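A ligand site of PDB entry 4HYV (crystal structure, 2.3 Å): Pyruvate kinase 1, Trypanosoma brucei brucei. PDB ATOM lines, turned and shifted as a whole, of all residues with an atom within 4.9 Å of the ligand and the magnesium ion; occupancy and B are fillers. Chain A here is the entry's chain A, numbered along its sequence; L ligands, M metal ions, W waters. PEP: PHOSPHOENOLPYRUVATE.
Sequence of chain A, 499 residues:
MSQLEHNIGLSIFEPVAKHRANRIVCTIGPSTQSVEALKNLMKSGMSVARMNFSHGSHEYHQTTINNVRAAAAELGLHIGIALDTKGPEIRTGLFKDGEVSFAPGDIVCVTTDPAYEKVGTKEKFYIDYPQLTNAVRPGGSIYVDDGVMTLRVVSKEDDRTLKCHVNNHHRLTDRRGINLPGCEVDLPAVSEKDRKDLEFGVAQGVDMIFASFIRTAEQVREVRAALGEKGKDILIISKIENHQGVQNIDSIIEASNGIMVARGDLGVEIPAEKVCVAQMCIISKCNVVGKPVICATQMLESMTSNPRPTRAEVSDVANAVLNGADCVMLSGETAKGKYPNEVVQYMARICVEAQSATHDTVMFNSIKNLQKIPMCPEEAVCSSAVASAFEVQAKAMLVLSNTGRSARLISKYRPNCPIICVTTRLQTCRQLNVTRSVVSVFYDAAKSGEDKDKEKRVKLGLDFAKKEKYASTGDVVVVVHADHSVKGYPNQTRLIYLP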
ATOM      1  N   ARG A  50       5.984   6.350 -34.549  1.00  0.00           N
ATOM      2  CA  ARG A  50       6.769   5.152 -34.166  1.00  0.00           C
ATOM      3  C   ARG A  50       5.867   4.118 -33.516  1.00  0.00           C
ATOM      4  O   ARG A  50       5.061   4.447 -32.626  1.00  0.00           O
ATOM      5  CB  ARG A  50       7.899   5.545 -33.207  1.00  0.00           C
ATOM      6  CG  ARG A  50       8.457   4.424 -32.357  1.00  0.00           C
ATOM      7  CD  ARG A  50       9.445   4.990 -31.336  1.00  0.00           C
ATOM      8  NE  ARG A  50      10.157   3.949 -30.608  1.00  0.00           N
ATOM      9  CZ  ARG A  50       9.955   3.647 -29.314  1.00  0.00           C
ATOM     10  NH1 ARG A  50       9.120   4.373 -28.568  1.00  0.00           N
ATOM     11  NH2 ARG A  50      10.674   2.667 -28.745  1.00  0.00           N
ATOM     12  N   ASN A  52       5.932   0.798 -31.313  1.00  0.00           N
ATOM     13  CA  ASN A  52       6.859   0.129 -30.450  1.00  0.00           C
ATOM     14  C   ASN A  52       6.460  -1.332 -30.261  1.00  0.00           C
ATOM     15  O   ASN A  52       5.534  -1.649 -29.511  1.00  0.00           O
ATOM     16  CB  ASN A  52       6.927   0.825 -29.116  1.00  0.00           C
ATOM     17  CG  ASN A  52       7.903   0.149 -28.176  1.00  0.00           C
ATOM     18  OD1 ASN A  52       8.682  -0.730 -28.581  1.00  0.00           O
ATOM     19  ND2 ASN A  52       7.861   0.539 -26.923  1.00  0.00           N
ATOM     20  N   SER A  54       7.718  -3.695 -28.827  1.00  0.00           N
ATOM     21  CA  SER A  54       7.805  -4.245 -27.493  1.00  0.00           C
ATOM     22  C   SER A  54       6.464  -4.677 -26.933  1.00  0.00           C
ATOM     23  O   SER A  54       6.405  -5.529 -26.049  1.00  0.00           O
ATOM     24  CB  SER A  54       8.489  -3.280 -26.565  1.00  0.00           C
ATOM     25  OG  SER A  54       9.862  -3.298 -26.838  1.00  0.00           O
ATOM     26  N   ASP A  84       9.541  -0.121 -34.573  1.00  0.00           N
ATOM     27  CA  ASP A  84      10.626  -0.190 -33.601  1.00  0.00           C
ATOM     28  C   ASP A  84      10.580  -1.583 -32.994  1.00  0.00           C
ATOM     29  O   ASP A  84       9.538  -2.010 -32.467  1.00  0.00           O
ATOM     30  CB  ASP A  84      10.439   0.887 -32.520  1.00  0.00           C
ATOM     31  CG  ASP A  84      11.572   0.935 -31.512  1.00  0.00           C
ATOM     32  OD1 ASP A  84      11.895  -0.134 -30.950  1.00  0.00           O
ATOM     33  OD2 ASP A  84      12.140   2.038 -31.259  1.00  0.00           O
ATOM     34  N   SER A 212      16.382  -2.346 -32.386  1.00  0.00           N
ATOM     35  CA  SER A 212      16.817  -2.257 -31.020  1.00  0.00           C
ATOM     36  C   SER A 212      18.125  -3.020 -30.781  1.00  0.00           C
ATOM     37  O   SER A 212      18.377  -4.073 -31.407  1.00  0.00           O
ATOM     38  CB  SER A 212      15.720  -2.723 -30.073  1.00  0.00           C
ATOM     39  OG  SER A 212      14.535  -1.977 -30.241  1.00  0.00           O
ATOM     40  N   PHE A 213      18.960  -2.479 -29.890  1.00  0.00           N
ATOM     41  CA  PHE A 213      20.148  -3.199 -29.377  1.00  0.00           C
ATOM     42  C   PHE A 213      21.180  -3.579 -30.416  1.00  0.00           C
ATOM     43  O   PHE A 213      21.936  -4.531 -30.221  1.00  0.00           O
ATOM     44  CB  PHE A 213      19.755  -4.417 -28.526  1.00  0.00           C
ATOM     45  CG  PHE A 213      18.924  -4.061 -27.309  1.00  0.00           C
ATOM     46  CD1 PHE A 213      19.515  -3.428 -26.214  1.00  0.00           C
ATOM     47  CD2 PHE A 213      17.525  -4.263 -27.305  1.00  0.00           C
ATOM     48  CE1 PHE A 213      18.732  -3.017 -25.120  1.00  0.00           C
ATOM     49  CE2 PHE A 213      16.749  -3.870 -26.212  1.00  0.00           C
ATOM     50  CZ  PHE A 213      17.353  -3.231 -25.120  1.00  0.00           C
ATOM     51  N   LYS A 239      19.581   1.420 -33.316  1.00  0.00           N
ATOM     52  CA  LYS A 239      19.475   2.052 -32.014  1.00  0.00           C
ATOM     53  C   LYS A 239      20.723   1.696 -31.195  1.00  0.00           C
ATOM     54  O   LYS A 239      21.066   0.531 -31.075  1.00  0.00           O
ATOM     55  CB  LYS A 239      18.208   1.585 -31.309  1.00  0.00           C
ATOM     56  CG  LYS A 239      16.934   2.101 -31.951  1.00  0.00           C
ATOM     57  CD  LYS A 239      15.716   1.293 -31.501  1.00  0.00           C
ATOM     58  CE  LYS A 239      15.530   1.353 -29.978  1.00  0.00           C
ATOM     59  NZ  LYS A 239      14.223   0.721 -29.605  1.00  0.00           N
ATOM     60  N   GLU A 241      22.268   1.457 -27.777  1.00  0.00           N
ATOM     61  CA  GLU A 241      21.785   1.387 -26.437  1.00  0.00           C
ATOM     62  C   GLU A 241      22.510   0.355 -25.611  1.00  0.00           C
ATOM     63  O   GLU A 241      22.091   0.038 -24.508  1.00  0.00           O
ATOM     64  CB  GLU A 241      20.248   1.175 -26.387  1.00  0.00           C
ATOM     65  CG  GLU A 241      19.703   0.155 -27.348  1.00  0.00           C
ATOM     66  CD  GLU A 241      18.193   0.075 -27.294  1.00  0.00           C
ATOM     67  OE1 GLU A 241      17.578   0.617 -26.331  1.00  0.00           O
ATOM     68  OE2 GLU A 241      17.605  -0.574 -28.196  1.00  0.00           O
ATOM     69  N   MET A 260      19.771   5.897 -33.972  1.00  0.00           N
ATOM     70  CA  MET A 260      19.095   6.484 -32.832  1.00  0.00           C
ATOM     71  C   MET A 260      19.977   6.391 -31.613  1.00  0.00           C
ATOM     72  O   MET A 260      20.466   5.317 -31.283  1.00  0.00           O
ATOM     73  CB  MET A 260      17.795   5.753 -32.553  1.00  0.00           C
ATOM     74  CG  MET A 260      16.914   6.491 -31.548  1.00  0.00           C
ATOM     75  SD  MET A 260      15.646   5.442 -30.860  1.00  0.00           S
ATOM     76  CE  MET A 260      14.475   5.440 -32.220  1.00  0.00           C
ATOM     77  N   ALA A 262      19.678   5.799 -28.240  1.00  0.00           N
ATOM     78  CA  ALA A 262      18.536   5.255 -27.523  1.00  0.00           C
ATOM     79  C   ALA A 262      18.816   5.360 -26.013  1.00  0.00           C
ATOM     80  O   ALA A 262      19.313   4.410 -25.411  1.00  0.00           O
ATOM     81  CB  ALA A 262      18.302   3.799 -27.931  1.00  0.00           C
ATOM     82  N   ARG A 263      18.603   6.559 -25.459  1.00  0.00           N
ATOM     83  CA  ARG A 263      19.250   6.941 -24.224  1.00  0.00           C
ATOM     84  C   ARG A 263      18.704   6.151 -23.028  1.00  0.00           C
ATOM     85  O   ARG A 263      19.361   6.051 -22.013  1.00  0.00           O
ATOM     86  CB  ARG A 263      19.122   8.458 -23.993  1.00  0.00           C
ATOM     87  CG  ARG A 263      19.957   9.317 -24.984  1.00  0.00           C
ATOM     88  CD  ARG A 263      19.942  10.793 -24.587  1.00  0.00           C
ATOM     89  NE  ARG A 263      18.580  11.269 -24.335  1.00  0.00           N
ATOM     90  CZ  ARG A 263      18.301  12.508 -23.955  1.00  0.00           C
ATOM     91  NH1 ARG A 263      19.275  13.402 -23.872  1.00  0.00           N
ATOM     92  NH2 ARG A 263      17.040  12.862 -23.673  1.00  0.00           N
ATOM     93  N   GLY A 264      17.506   5.580 -23.170  1.00  0.00           N
ATOM     94  CA  GLY A 264      16.846   4.858 -22.081  1.00  0.00           C
ATOM     95  C   GLY A 264      17.629   3.603 -21.684  1.00  0.00           C
ATOM     96  O   GLY A 264      18.266   3.579 -20.629  1.00  0.00           O
ATOM     97  N   ASP A 265      17.693   2.610 -22.577  1.00  0.00           N
ATOM     98  CA  ASP A 265      18.593   1.486 -22.330  1.00  0.00           C
ATOM     99  C   ASP A 265      20.063   1.874 -22.209  1.00  0.00           C
ATOM    100  O   ASP A 265      20.781   1.351 -21.336  1.00  0.00           O
ATOM    101  CB  ASP A 265      18.387   0.360 -23.353  1.00  0.00           C
ATOM    102  CG  ASP A 265      17.088  -0.413 -23.089  1.00  0.00           C
ATOM    103  OD1 ASP A 265      16.076  -0.126 -23.787  1.00  0.00           O
ATOM    104  OD2 ASP A 265      17.034  -1.120 -22.062  1.00  0.00           O
ATOM    105  N   LEU A 266      20.520   2.811 -23.037  1.00  0.00           N
ATOM    106  CA  LEU A 266      21.935   3.191 -22.978  1.00  0.00           C
ATOM    107  C   LEU A 266      22.345   3.605 -21.570  1.00  0.00           C
ATOM    108  O   LEU A 266      23.457   3.330 -21.114  1.00  0.00           O
ATOM    109  CB  LEU A 266      22.240   4.305 -23.971  1.00  0.00           C
ATOM    110  CG  LEU A 266      23.696   4.732 -24.128  1.00  0.00           C
ATOM    111  CD1 LEU A 266      24.507   3.521 -24.598  1.00  0.00           C
ATOM    112  CD2 LEU A 266      23.791   5.876 -25.155  1.00  0.00           C
ATOM    113  N   ALA A 296      16.697  10.244 -28.502  1.00  0.00           N
ATOM    114  CA  ALA A 296      15.507   9.635 -27.913  1.00  0.00           C
ATOM    115  C   ALA A 296      15.540   9.550 -26.381  1.00  0.00           C
ATOM    116  O   ALA A 296      16.584   9.407 -25.782  1.00  0.00           O
ATOM    117  CB  ALA A 296      15.254   8.252 -28.504  1.00  0.00           C
ATOM    118  N   THR A 297      14.353   9.679 -25.789  1.00  0.00           N
ATOM    119  CA  THR A 297      13.981   9.059 -24.508  1.00  0.00           C
ATOM    120  C   THR A 297      14.093  10.029 -23.317  1.00  0.00           C
ATOM    121  O   THR A 297      15.134  10.633 -23.088  1.00  0.00           O
ATOM    122  CB  THR A 297      14.717   7.748 -24.210  1.00  0.00           C
ATOM    123  OG1 THR A 297      14.422   6.746 -25.231  1.00  0.00           O
ATOM    124  CG2 THR A 297      14.291   7.225 -22.804  1.00  0.00           C
ATOM    125  N   MET A 329      12.823  12.766 -30.262  1.00  0.00           N
ATOM    126  CA  MET A 329      11.778  11.767 -30.132  1.00  0.00           C
ATOM    127  C   MET A 329      10.974  11.852 -28.812  1.00  0.00           C
ATOM    128  O   MET A 329      11.484  12.278 -27.783  1.00  0.00           O
ATOM    129  CB  MET A 329      12.371  10.386 -30.282  1.00  0.00           C
ATOM    130  CG  MET A 329      11.324   9.291 -30.325  1.00  0.00           C
ATOM    131  SD  MET A 329      12.056   7.758 -30.925  1.00  0.00           S
ATOM    132  CE  MET A 329      12.146   6.819 -29.400  1.00  0.00           C
HETATM  133  C1  PEP L   1      15.634   3.579 -25.553  1.00  0.00           C
HETATM  134  O1  PEP L   1      16.013   2.600 -24.850  1.00  0.00           O
HETATM  135  O2' PEP L   1      16.070   4.735 -25.326  1.00  0.00           O
HETATM  136  C2  PEP L   1      14.578   3.373 -26.632  1.00  0.00           C
HETATM  137  C3  PEP L   1      14.303   4.494 -27.663  1.00  0.00           C
HETATM  138  O2  PEP L   1      14.167   2.112 -26.907  1.00  0.00           O
HETATM  139  P   PEP L   1      12.960   1.358 -25.999  1.00  0.00           P
HETATM  140  O1P PEP L   1      12.123   0.763 -27.171  1.00  0.00           O
HETATM  141  O2P PEP L   1      13.643   0.708 -24.862  1.00  0.00           O
HETATM  142  O3P PEP L   1      12.016   2.492 -25.455  1.00  0.00           O
HETATM  143 MG    MG M   1      15.648   0.567 -25.503  1.00  0.00          MG
HETATM  144  O   HOH W   1      10.393  -0.584 -25.436  1.00  0.00           O
HETATM  145  O   HOH W   2       9.572   3.294 -25.708  1.00  0.00           O
HETATM  146  O   HOH W   3      15.297  -0.747 -27.019  1.00  0.00           O
HETATM  147  O   HOH W   4      11.867   5.397 -25.221  1.00  0.00           O
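N of Asp 265 lies close to O1 of the ligand (2.8 Å). The guanidinium group (NH2) of Arg 50 lies within salt-bridge range of an oxygen (O1P) of the ligand (2.9 Å). An oxygen (O2') of the ligand lies within hydrogen-bond range of the backbone NH (N) of Gly 264 (2.7 Å). The backbone NH (N) of Arg 263 sits at hydrogen-bond distance from an oxygen (O2') of the ligand (3.1 Å). The side-chain amino group of Lys 239 lies within salt-bridge range of an oxygen (O1P) of the ligand, at 3.2 Å. The side-chain hydroxyl of Thr 297 lies within hydrogen-bond range of an oxygen (O2') of the ligand (2.6 Å).
NZ of Lys 239 lies within hydrogen-bond range of OG of Ser 212, 2.8 Å away. O of Ala 296 sits at hydrogen-bond distance from NE of Arg 263, at 3.1 Å. NE of Arg 50 is in salt-bridge range of OD2 of Asp 84 (2.8 Å). NZ of Lys 239 is in salt-bridge range of OD1 of Asp 84, at 2.8 Å. The side-chain carboxylate of Glu 241 is in salt-bridge range of the side-chain amino group of Lys 239, at 3.9 Å. OD1 of Asp 84 lies within hydrogen-bond range of OG of Ser 212, at 3.3 Å. The backbone carbonyl oxygen (O) of Thr 297 lies within hydrogen-bond range of the guanidinium group (NH2) of Arg 263. The backbone NH (N) of Phe 213 is in hydrogen-bond range of the side-chain carboxylate (OE2) of Glu 241, 2.9 Å away.
The backbone carbonyl oxygen (O) of Ala 262 lies close to an oxygen (O2') of the ligand (3.3 Å). Merely in contact with the ligand: Met 260, Met 329, Asp 84 and Ala 296. Hydrophobic or aromatic side chains within 4 Å of the ligand: Met 260, Ala 262, Ala 296 and Met 329. Within 4 Å of the ligand: Arg 50, Asp 84, Lys 239, Glu 241, Met 260, Ala 262, Arg 263, Gly 264, Asp 265, Ala 296, Thr 297 and Met 329. The nearest printed residue that does not touch the ligand is Asn 52 (4.01 Å).
The nearest printed residue that does not touch the magnesium ion is Phe 213 (4.2 Å).
The magnesium ion is bound by the side-chain carboxylate of Asp 265, water W3, the side-chain carboxylate of Glu 241, an oxygen (O2P) of the ligand, an oxygen (O1) of the ligand and an oxygen (O2) of the ligand.
Water W3 lies within hydrogen-bond range of OE2 of Glu 241 (2.6 Å) and NZ of Lys 239 (3.2 Å). Water W2 lies within hydrogen-bond range of O3P of the ligand, NH1 of Arg 50 and ND2 of Asn 52. Water W1 lies within hydrogen-bond range of O1P of the ligand (2.8 Å), OG of Ser 54 (3.1 Å) and ND2 of Asn 52 (3.1 Å). Water W4 bridges the side-chain hydroxyl of Thr 297 (2.9 Å) and an oxygen (O3P) of the ligand (2.9 Å).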
